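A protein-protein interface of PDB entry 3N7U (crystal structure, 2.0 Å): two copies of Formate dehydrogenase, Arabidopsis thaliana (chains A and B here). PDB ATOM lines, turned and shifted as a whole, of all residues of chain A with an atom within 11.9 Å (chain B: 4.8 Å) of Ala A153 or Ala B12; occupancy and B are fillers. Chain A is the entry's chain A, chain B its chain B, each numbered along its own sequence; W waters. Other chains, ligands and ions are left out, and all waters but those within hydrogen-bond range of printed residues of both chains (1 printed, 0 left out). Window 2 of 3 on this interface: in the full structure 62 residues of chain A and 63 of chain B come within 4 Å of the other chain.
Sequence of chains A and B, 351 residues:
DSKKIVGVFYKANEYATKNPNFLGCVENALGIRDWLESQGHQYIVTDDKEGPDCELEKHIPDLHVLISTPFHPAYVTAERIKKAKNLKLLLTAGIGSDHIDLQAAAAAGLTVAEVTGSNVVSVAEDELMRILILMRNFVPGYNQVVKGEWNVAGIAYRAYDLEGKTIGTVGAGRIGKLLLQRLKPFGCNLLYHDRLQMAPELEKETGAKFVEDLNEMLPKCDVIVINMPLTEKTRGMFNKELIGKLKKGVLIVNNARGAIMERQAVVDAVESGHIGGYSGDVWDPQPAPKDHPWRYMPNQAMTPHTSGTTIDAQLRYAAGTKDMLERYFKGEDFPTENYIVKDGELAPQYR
N of Ala A153 lies close to OD1 of Asn A151 (3.5 Å).
The backbone NH (N) of Asn A151 is in hydrogen-bond range of the side-chain amide oxygen (OE1) of Gln A144, at 2.8 Å.
The side-chain carboxylate (OE1) of Glu B27 is in hydrogen-bond range of the backbone NH (N) of Ala B12 (3.0 Å).
The backbone NH of Gly A154 lies within hydrogen-bond range of the side-chain amide oxygen of Asn A151, 3.5 Å away.
The backbone carbonyl oxygen of Phe B22 sits at hydrogen-bond distance from the side-chain sulfur of Cys B25 (3.5 Å).
Asn A151 touches Tyr B15.
Tyr B10 touches Val A152 (CZ to CG1, 3.9 Å).
Ala A153 touches Lys B11 (CB to O, 3.8 Å).
Ala A153 touches Ala B12 (CB to CA, 3.5 Å).
Tyr B15 touches Ala A153.
Phe B22 touches Ala A153 (CZ to CB, 3.7 Å).
Gly A154 touches Tyr B15.
Tyr B10 touches Ala A156 (OH to CB, 3.8 Å).
Tyr A157 touches Tyr B15 (CD2 to CD2, 3.6 Å).
Phe B22 touches Tyr A157 (CE1 to CB, 3.5 Å).
Ala A153 touches four residues of chain B.
Ile A155 touches none of the printed residues of chain B.
Printed residues of chain B within 4 Å of Ala A156: Tyr B10 (3.8 Å).
Printed residues of chain B within 4 Å of Tyr A157: Tyr B15 (3.6 Å) and Phe B22 (3.5 Å).
Of the printed residues of chain A, Tyr B10 touches Val A152 and Ala A156.
Lys B11 touches just one residue of chain A: Ala A153 (3.8 Å).
Of chain A, only Ala A153 comes within 4 Å of Ala B12.
No residue of chain A comes within 4 Å of Asn B13.
No residue of chain A comes within 4 Å of Ala B16.
Cys B25 touches none of the printed residues of chain A.
The nearest residue of chain B that does not touch Ala A153 is Tyr B10 (4.03 Å).
The nearest residue of chain A that does not touch Ala B12 is Asn A151 (5.6 Å).
Printed residues of chain B that touch a printed residue of chain A: Tyr B10, Lys B11, Ala B12, Tyr B15 and Phe B22.
No position is printed for both chains.
Water W1 lies within hydrogen-bond range of O of Lys B11, OD1 of Asn A151, N of Ala A153 and N of Val A152.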
ATOM      1  N   MET A 135     -11.515   8.404  -5.200  1.00  0.00           N
ATOM      2  CA  MET A 135     -11.449   9.709  -5.944  1.00  0.00           C
ATOM      3  C   MET A 135     -11.501  10.888  -4.981  1.00  0.00           C
ATOM      4  O   MET A 135     -10.674  11.769  -5.047  1.00  0.00           O
ATOM      5  CB  MET A 135     -12.561   9.810  -6.998  1.00  0.00           C
ATOM      6  CG  MET A 135     -12.508  11.020  -8.006  1.00  0.00           C
ATOM      7  SD  MET A 135     -10.941  10.959  -8.950  1.00  0.00           S
ATOM      8  CE  MET A 135     -11.304   9.671 -10.131  1.00  0.00           C
ATOM      9  N   ARG A 136     -12.441  10.834  -4.043  1.00  0.00           N
ATOM     10  CA  ARG A 136     -12.803  11.935  -3.129  1.00  0.00           C
ATOM     11  C   ARG A 136     -12.011  11.831  -1.796  1.00  0.00           C
ATOM     12  O   ARG A 136     -12.086  12.717  -0.909  1.00  0.00           O
ATOM     13  CB  ARG A 136     -14.349  11.938  -2.897  1.00  0.00           C
ATOM     14  CG  ARG A 136     -15.251  11.935  -4.166  1.00  0.00           C
ATOM     15  CD  ARG A 136     -16.764  12.367  -3.897  1.00  0.00           C
ATOM     16  NE  ARG A 136     -16.711  13.594  -3.123  1.00  0.00           N
ATOM     17  CZ  ARG A 136     -16.598  14.827  -3.641  1.00  0.00           C
ATOM     18  NH1 ARG A 136     -16.667  15.058  -4.958  1.00  0.00           N
ATOM     19  NH2 ARG A 136     -16.446  15.823  -2.809  1.00  0.00           N
ATOM     20  N   ASN A 137     -11.204  10.769  -1.680  1.00  0.00           N
ATOM     21  CA  ASN A 137     -10.262  10.602  -0.564  1.00  0.00           C
ATOM     22  C   ASN A 137     -10.901  10.532   0.859  1.00  0.00           C
ATOM     23  O   ASN A 137     -10.440  11.206   1.803  1.00  0.00           O
ATOM     24  CB  ASN A 137      -9.175  11.698  -0.627  1.00  0.00           C
ATOM     25  CG  ASN A 137      -7.853  11.235  -0.063  1.00  0.00           C
ATOM     26  OD1 ASN A 137      -7.514  10.039  -0.151  1.00  0.00           O
ATOM     27  ND2 ASN A 137      -7.064  12.179   0.507  1.00  0.00           N
ATOM     28  N   PHE A 138     -11.934   9.703   0.998  1.00  0.00           N
ATOM     29  CA  PHE A 138     -12.647   9.548   2.270  1.00  0.00           C
ATOM     30  C   PHE A 138     -11.794   8.943   3.371  1.00  0.00           C
ATOM     31  O   PHE A 138     -11.834   9.426   4.505  1.00  0.00           O
ATOM     32  CB  PHE A 138     -13.909   8.676   2.070  1.00  0.00           C
ATOM     33  CG  PHE A 138     -14.585   8.263   3.369  1.00  0.00           C
ATOM     34  CD1 PHE A 138     -15.474   9.149   4.026  1.00  0.00           C
ATOM     35  CD2 PHE A 138     -14.339   7.005   3.923  1.00  0.00           C
ATOM     36  CE1 PHE A 138     -16.112   8.795   5.241  1.00  0.00           C
ATOM     37  CE2 PHE A 138     -14.954   6.603   5.133  1.00  0.00           C
ATOM     38  CZ  PHE A 138     -15.861   7.493   5.805  1.00  0.00           C
ATOM     39  N   PRO A 140      -8.483   8.835   4.475  1.00  0.00           N
ATOM     40  CA  PRO A 140      -7.646   9.698   5.319  1.00  0.00           C
ATOM     41  C   PRO A 140      -8.445  10.682   6.208  1.00  0.00           C
ATOM     42  O   PRO A 140      -7.994  11.016   7.316  1.00  0.00           O
ATOM     43  CB  PRO A 140      -6.797  10.469   4.306  1.00  0.00           C
ATOM     44  CG  PRO A 140      -6.740   9.601   3.115  1.00  0.00           C
ATOM     45  CD  PRO A 140      -8.104   8.922   3.053  1.00  0.00           C
ATOM     46  N   GLY A 141      -9.617  11.133   5.756  1.00  0.00           N
ATOM     47  CA  GLY A 141     -10.501  11.954   6.636  1.00  0.00           C
ATOM     48  C   GLY A 141     -11.059  11.227   7.847  1.00  0.00           C
ATOM     49  O   GLY A 141     -11.118  11.780   8.956  1.00  0.00           O
ATOM     50  N   GLN A 144      -8.165  10.693  10.427  1.00  0.00           N
ATOM     51  CA  GLN A 144      -7.994  11.914  11.209  1.00  0.00           C
ATOM     52  C   GLN A 144      -9.062  12.048  12.293  1.00  0.00           C
ATOM     53  O   GLN A 144      -8.767  12.466  13.425  1.00  0.00           O
ATOM     54  CB  GLN A 144      -8.067  13.183  10.322  1.00  0.00           C
ATOM     55  CG  GLN A 144      -6.804  13.452   9.494  1.00  0.00           C
ATOM     56  CD  GLN A 144      -6.826  14.807   8.758  1.00  0.00           C
ATOM     57  OE1 GLN A 144      -7.591  15.703   9.106  1.00  0.00           O
ATOM     58  NE2 GLN A 144      -5.949  14.964   7.771  1.00  0.00           N
ATOM     59  N   GLU A 149      -7.372  14.220  15.190  1.00  0.00           N
ATOM     60  CA  GLU A 149      -6.673  15.204  14.370  1.00  0.00           C
ATOM     61  C   GLU A 149      -7.616  16.136  13.557  1.00  0.00           C
ATOM     62  O   GLU A 149      -8.842  15.924  13.519  1.00  0.00           O
ATOM     63  CB  GLU A 149      -5.685  14.504  13.406  1.00  0.00           C
ATOM     64  CG  GLU A 149      -4.619  13.662  14.077  1.00  0.00           C
ATOM     65  CD  GLU A 149      -3.837  12.776  13.093  1.00  0.00           C
ATOM     66  OE1 GLU A 149      -4.249  12.531  11.955  1.00  0.00           O
ATOM     67  OE2 GLU A 149      -2.784  12.276  13.469  1.00  0.00           O
ATOM     68  N   TRP A 150      -7.027  17.148  12.885  1.00  0.00           N
ATOM     69  CA  TRP A 150      -7.780  18.045  11.939  1.00  0.00           C
ATOM     70  C   TRP A 150      -6.819  18.730  10.988  1.00  0.00           C
ATOM     71  O   TRP A 150      -6.124  19.662  11.388  1.00  0.00           O
ATOM     72  CB  TRP A 150      -8.634  19.089  12.677  1.00  0.00           C
ATOM     73  CG  TRP A 150      -9.505  19.977  11.743  1.00  0.00           C
ATOM     74  CD1 TRP A 150      -9.065  21.047  10.989  1.00  0.00           C
ATOM     75  CD2 TRP A 150     -10.920  19.855  11.462  1.00  0.00           C
ATOM     76  NE1 TRP A 150     -10.114  21.596  10.276  1.00  0.00           N
ATOM     77  CE2 TRP A 150     -11.259  20.894  10.544  1.00  0.00           C
ATOM     78  CE3 TRP A 150     -11.933  19.009  11.916  1.00  0.00           C
ATOM     79  CZ2 TRP A 150     -12.562  21.095  10.071  1.00  0.00           C
ATOM     80  CZ3 TRP A 150     -13.258  19.214  11.426  1.00  0.00           C
ATOM     81  CH2 TRP A 150     -13.542  20.246  10.504  1.00  0.00           C
ATOM     82  N   ASN A 151      -6.778  18.293   9.736  1.00  0.00           N
ATOM     83  CA  ASN A 151      -5.849  18.862   8.720  1.00  0.00           C
ATOM     84  C   ASN A 151      -6.457  18.732   7.350  1.00  0.00           C
ATOM     85  O   ASN A 151      -6.150  17.783   6.631  1.00  0.00           O
ATOM     86  CB  ASN A 151      -4.476  18.103   8.728  1.00  0.00           C
ATOM     87  CG  ASN A 151      -3.434  18.735   7.789  1.00  0.00           C
ATOM     88  OD1 ASN A 151      -3.672  19.777   7.177  1.00  0.00           O
ATOM     89  ND2 ASN A 151      -2.278  18.090   7.657  1.00  0.00           N
ATOM     90  N   VAL A 152      -7.315  19.682   6.959  1.00  0.00           N
ATOM     91  CA  VAL A 152      -7.975  19.625   5.646  1.00  0.00           C
ATOM     92  C   VAL A 152      -7.003  19.479   4.476  1.00  0.00           C
ATOM     93  O   VAL A 152      -7.292  18.771   3.502  1.00  0.00           O
ATOM     94  CB  VAL A 152      -8.969  20.844   5.429  1.00  0.00           C
ATOM     95  CG1 VAL A 152      -9.516  20.916   3.981  1.00  0.00           C
ATOM     96  CG2 VAL A 152     -10.126  20.779   6.472  1.00  0.00           C
ATOM     97  N   ALA A 153      -5.867  20.178   4.537  1.00  0.00           N
ATOM     98  CA  ALA A 153      -4.906  20.115   3.401  1.00  0.00           C
ATOM     99  C   ALA A 153      -4.345  18.737   3.156  1.00  0.00           C
ATOM    100  O   ALA A 153      -4.082  18.366   2.011  1.00  0.00           O
ATOM    101  CB  ALA A 153      -3.759  21.130   3.586  1.00  0.00           C
ATOM    102  N   GLY A 154      -4.166  17.975   4.222  1.00  0.00           N
ATOM    103  CA  GLY A 154      -3.658  16.604   4.146  1.00  0.00           C
ATOM    104  C   GLY A 154      -4.588  15.677   3.389  1.00  0.00           C
ATOM    105  O   GLY A 154      -4.180  14.597   2.967  1.00  0.00           O
ATOM    106  N   ILE A 155      -5.835  16.122   3.209  1.00  0.00           N
ATOM    107  CA  ILE A 155      -6.859  15.415   2.434  1.00  0.00           C
ATOM    108  C   ILE A 155      -7.104  16.091   1.078  1.00  0.00           C
ATOM    109  O   ILE A 155      -7.158  15.428   0.040  1.00  0.00           O
ATOM    110  CB  ILE A 155      -8.201  15.360   3.244  1.00  0.00           C
ATOM    111  CG1 ILE A 155      -7.982  14.591   4.568  1.00  0.00           C
ATOM    112  CG2 ILE A 155      -9.283  14.707   2.427  1.00  0.00           C
ATOM    113  CD1 ILE A 155      -8.872  15.022   5.786  1.00  0.00           C
ATOM    114  N   ALA A 156      -7.236  17.419   1.072  1.00  0.00           N
ATOM    115  CA  ALA A 156      -7.707  18.114  -0.136  1.00  0.00           C
ATOM    116  C   ALA A 156      -6.717  18.082  -1.321  1.00  0.00           C
ATOM    117  O   ALA A 156      -7.147  18.131  -2.489  1.00  0.00           O
ATOM    118  CB  ALA A 156      -8.113  19.557   0.184  1.00  0.00           C
ATOM    119  N   TYR A 157      -5.412  17.988  -1.034  1.00  0.00           N
ATOM    120  CA  TYR A 157      -4.397  18.087  -2.080  1.00  0.00           C
ATOM    121  C   TYR A 157      -4.605  17.030  -3.165  1.00  0.00           C
ATOM    122  O   TYR A 157      -4.197  17.243  -4.314  1.00  0.00           O
ATOM    123  CB  TYR A 157      -2.961  18.047  -1.488  1.00  0.00           C
ATOM    124  CG  TYR A 157      -2.454  16.644  -1.201  1.00  0.00           C
ATOM    125  CD1 TYR A 157      -1.809  15.886  -2.192  1.00  0.00           C
ATOM    126  CD2 TYR A 157      -2.581  16.096   0.070  1.00  0.00           C
ATOM    127  CE1 TYR A 157      -1.320  14.601  -1.907  1.00  0.00           C
ATOM    128  CE2 TYR A 157      -2.133  14.822   0.353  1.00  0.00           C
ATOM    129  CZ  TYR A 157      -1.514  14.082  -0.627  1.00  0.00           C
ATOM    130  OH  TYR A 157      -1.088  12.821  -0.274  1.00  0.00           O
ATOM    131  N   ARG A 158      -5.221  15.893  -2.815  1.00  0.00           N
ATOM    132  CA  ARG A 158      -5.449  14.805  -3.784  1.00  0.00           C
ATOM    133  C   ARG A 158      -6.927  14.355  -3.913  1.00  0.00           C
ATOM    134  O   ARG A 158      -7.191  13.305  -4.505  1.00  0.00           O
ATOM    135  CB  ARG A 158      -4.515  13.595  -3.547  1.00  0.00           C
ATOM    136  CG  ARG A 158      -4.641  12.956  -2.147  1.00  0.00           C
ATOM    137  CD  ARG A 158      -3.937  11.598  -2.039  1.00  0.00           C
ATOM    138  NE  ARG A 158      -4.679  10.501  -2.673  1.00  0.00           N
ATOM    139  CZ  ARG A 158      -4.144   9.328  -3.065  1.00  0.00           C
ATOM    140  NH1 ARG A 158      -2.835   9.102  -2.916  1.00  0.00           N
ATOM    141  NH2 ARG A 158      -4.921   8.384  -3.616  1.00  0.00           N
ATOM    142  N   ALA A 159      -7.858  15.141  -3.375  1.00  0.00           N
ATOM    143  CA  ALA A 159      -9.298  14.929  -3.572  1.00  0.00           C
ATOM    144  C   ALA A 159      -9.854  15.626  -4.858  1.00  0.00           C
ATOM    145  O   ALA A 159      -9.553  16.790  -5.113  1.00  0.00           O
ATOM    146  CB  ALA A 159     -10.021  15.410  -2.359  1.00  0.00           C
ATOM    147  N   TYR A 160     -10.665  14.892  -5.632  1.00  0.00           N
ATOM    148  CA  TYR A 160     -11.188  15.290  -6.921  1.00  0.00           C
ATOM    149  C   TYR A 160     -12.664  14.892  -7.015  1.00  0.00           C
ATOM    150  O   TYR A 160     -13.096  13.944  -6.331  1.00  0.00           O
ATOM    151  CB  TYR A 160     -10.443  14.543  -8.037  1.00  0.00           C
ATOM    152  CG  TYR A 160      -9.100  15.140  -8.397  1.00  0.00           C
ATOM    153  CD1 TYR A 160      -9.031  16.211  -9.299  1.00  0.00           C
ATOM    154  CD2 TYR A 160      -7.911  14.630  -7.874  1.00  0.00           C
ATOM    155  CE1 TYR A 160      -7.822  16.759  -9.677  1.00  0.00           C
ATOM    156  CE2 TYR A 160      -6.667  15.217  -8.225  1.00  0.00           C
ATOM    157  CZ  TYR A 160      -6.650  16.270  -9.143  1.00  0.00           C
ATOM    158  OH  TYR A 160      -5.481  16.884  -9.552  1.00  0.00           O
ATOM    159  N   ASN A 299      -2.604   4.174   1.216  1.00  0.00           N
ATOM    160  CA  ASN A 299      -3.823   4.511   0.472  1.00  0.00           C
ATOM    161  C   ASN A 299      -4.908   3.405   0.345  1.00  0.00           C
ATOM    162  O   ASN A 299      -5.910   3.585  -0.376  1.00  0.00           O
ATOM    163  CB  ASN A 299      -3.429   5.131  -0.885  1.00  0.00           C
ATOM    164  CG  ASN A 299      -2.527   6.374  -0.708  1.00  0.00           C
ATOM    165  OD1 ASN A 299      -2.897   7.312  -0.004  1.00  0.00           O
ATOM    166  ND2 ASN A 299      -1.332   6.350  -1.292  1.00  0.00           N
ATOM    167  N   TYR B  10      -7.211  27.529   5.058  1.00  0.00           N
ATOM    168  CA  TYR B  10      -6.532  26.488   5.838  1.00  0.00           C
ATOM    169  C   TYR B  10      -5.082  26.450   5.338  1.00  0.00           C
ATOM    170  O   TYR B  10      -4.824  26.657   4.137  1.00  0.00           O
ATOM    171  CB  TYR B  10      -7.219  25.105   5.692  1.00  0.00           C
ATOM    172  CG  TYR B  10      -7.586  24.668   4.281  1.00  0.00           C
ATOM    173  CD1 TYR B  10      -6.659  23.983   3.489  1.00  0.00           C
ATOM    174  CD2 TYR B  10      -8.866  24.918   3.746  1.00  0.00           C
ATOM    175  CE1 TYR B  10      -6.971  23.552   2.211  1.00  0.00           C
ATOM    176  CE2 TYR B  10      -9.201  24.506   2.446  1.00  0.00           C
ATOM    177  CZ  TYR B  10      -8.234  23.813   1.686  1.00  0.00           C
ATOM    178  OH  TYR B  10      -8.489  23.371   0.414  1.00  0.00           O
ATOM    179  N   LYS B  11      -4.171  26.153   6.263  1.00  0.00           N
ATOM    180  CA  LYS B  11      -2.723  26.110   5.997  1.00  0.00           C
ATOM    181  C   LYS B  11      -2.320  24.731   5.507  1.00  0.00           C
ATOM    182  O   LYS B  11      -2.718  23.743   6.115  1.00  0.00           O
ATOM    183  CB  LYS B  11      -1.946  26.466   7.280  1.00  0.00           C
ATOM    184  CG  LYS B  11      -0.425  26.633   7.074  1.00  0.00           C
ATOM    185  CD  LYS B  11       0.281  27.331   8.280  1.00  0.00           C
ATOM    186  CE  LYS B  11       0.268  26.425   9.521  1.00  0.00           C
ATOM    187  NZ  LYS B  11       0.901  27.044  10.711  1.00  0.00           N
ATOM    188  N   ALA B  12      -1.559  24.661   4.409  1.00  0.00           N
ATOM    189  CA  ALA B  12      -1.133  23.389   3.788  1.00  0.00           C
ATOM    190  C   ALA B  12       0.339  22.924   4.052  1.00  0.00           C
ATOM    191  O   ALA B  12       0.633  21.733   3.897  1.00  0.00           O
ATOM    192  CB  ALA B  12      -1.384  23.408   2.291  1.00  0.00           C
ATOM    193  N   ASN B  13       1.221  23.853   4.422  1.00  0.00           N
ATOM    194  CA  ASN B  13       2.683  23.603   4.513  1.00  0.00           C
ATOM    195  C   ASN B  13       3.186  22.791   3.299  1.00  0.00           C
ATOM    196  O   ASN B  13       2.996  23.226   2.138  1.00  0.00           O
ATOM    197  CB  ASN B  13       3.090  23.024   5.894  1.00  0.00           C
ATOM    198  CG  ASN B  13       3.043  24.071   7.005  1.00  0.00           C
ATOM    199  OD1 ASN B  13       3.059  25.267   6.734  1.00  0.00           O
ATOM    200  ND2 ASN B  13       3.013  23.634   8.254  1.00  0.00           N
ATOM    201  N   GLU B  14       3.771  21.613   3.540  1.00  0.00           N
ATOM    202  CA  GLU B  14       4.368  20.766   2.442  1.00  0.00           C
ATOM    203  C   GLU B  14       3.343  20.231   1.432  1.00  0.00           C
ATOM    204  O   GLU B  14       3.691  19.898   0.283  1.00  0.00           O
ATOM    205  CB  GLU B  14       5.217  19.595   3.008  1.00  0.00           C
ATOM    206  CG  GLU B  14       4.443  18.441   3.715  1.00  0.00           C
ATOM    207  CD  GLU B  14       4.110  18.729   5.193  1.00  0.00           C
ATOM    208  OE1 GLU B  14       3.768  17.777   5.925  1.00  0.00           O
ATOM    209  OE2 GLU B  14       4.165  19.897   5.639  1.00  0.00           O
ATOM    210  N   TYR B  15       2.077  20.153   1.851  1.00  0.00           N
ATOM    211  CA  TYR B  15       1.013  19.729   0.905  1.00  0.00           C
ATOM    212  C   TYR B  15       0.740  20.714  -0.246  1.00  0.00           C
ATOM    213  O   TYR B  15       0.286  20.287  -1.324  1.00  0.00           O
ATOM    214  CB  TYR B  15      -0.295  19.393   1.651  1.00  0.00           C
ATOM    215  CG  TYR B  15      -0.128  18.276   2.673  1.00  0.00           C
ATOM    216  CD1 TYR B  15      -0.202  18.546   4.041  1.00  0.00           C
ATOM    217  CD2 TYR B  15       0.122  16.963   2.277  1.00  0.00           C
ATOM    218  CE1 TYR B  15      -0.031  17.535   4.989  1.00  0.00           C
ATOM    219  CE2 TYR B  15       0.270  15.928   3.221  1.00  0.00           C
ATOM    220  CZ  TYR B  15       0.196  16.232   4.566  1.00  0.00           C
ATOM    221  OH  TYR B  15       0.340  15.248   5.513  1.00  0.00           O
ATOM    222  N   ALA B  16       1.025  22.006  -0.030  1.00  0.00           N
ATOM    223  CA  ALA B  16       0.664  23.073  -0.994  1.00  0.00           C
ATOM    224  C   ALA B  16       1.106  22.813  -2.437  1.00  0.00           C
ATOM    225  O   ALA B  16       0.356  23.016  -3.401  1.00  0.00           O
ATOM    226  CB  ALA B  16       1.159  24.425  -0.506  1.00  0.00           C
ATOM    227  N   PHE B  22      -3.846  23.443  -6.486  1.00  0.00           N
ATOM    228  CA  PHE B  22      -4.217  23.460  -5.060  1.00  0.00           C
ATOM    229  C   PHE B  22      -4.439  24.900  -4.573  1.00  0.00           C
ATOM    230  O   PHE B  22      -3.740  25.403  -3.708  1.00  0.00           O
ATOM    231  CB  PHE B  22      -3.167  22.664  -4.202  1.00  0.00           C
ATOM    232  CG  PHE B  22      -3.592  22.346  -2.750  1.00  0.00           C
ATOM    233  CD1 PHE B  22      -2.678  21.730  -1.883  1.00  0.00           C
ATOM    234  CD2 PHE B  22      -4.880  22.669  -2.242  1.00  0.00           C
ATOM    235  CE1 PHE B  22      -3.021  21.429  -0.550  1.00  0.00           C
ATOM    236  CE2 PHE B  22      -5.236  22.362  -0.906  1.00  0.00           C
ATOM    237  CZ  PHE B  22      -4.297  21.753  -0.059  1.00  0.00           C
ATOM    238  N   CYS B  25      -5.659  26.603  -0.336  1.00  0.00           N
ATOM    239  CA  CYS B  25      -4.824  26.761   0.881  1.00  0.00           C
ATOM    240  C   CYS B  25      -4.214  28.182   1.033  1.00  0.00           C
ATOM    241  O   CYS B  25      -4.199  28.954   0.057  1.00  0.00           O
ATOM    242  CB  CYS B  25      -3.685  25.694   0.927  1.00  0.00           C
ATOM    243  SG  CYS B  25      -2.517  25.768  -0.469  1.00  0.00           S
ATOM    244  N   GLU B  27      -1.059  29.126   1.207  1.00  0.00           N
ATOM    245  CA  GLU B  27       0.147  29.304   0.389  1.00  0.00           C
ATOM    246  C   GLU B  27      -0.145  29.753  -1.056  1.00  0.00           C
ATOM    247  O   GLU B  27       0.577  30.629  -1.579  1.00  0.00           O
ATOM    248  CB  GLU B  27       1.027  28.037   0.405  1.00  0.00           C
ATOM    249  CG  GLU B  27       1.557  27.648   1.821  1.00  0.00           C
ATOM    250  CD  GLU B  27       0.533  26.997   2.781  1.00  0.00           C
ATOM    251  OE1 GLU B  27      -0.624  26.672   2.401  1.00  0.00           O
ATOM    252  OE2 GLU B  27       0.884  26.820   3.964  1.00  0.00           O
HETATM  253  O   HOH W   1      -5.099  22.318   6.603  1.00  0.00           O
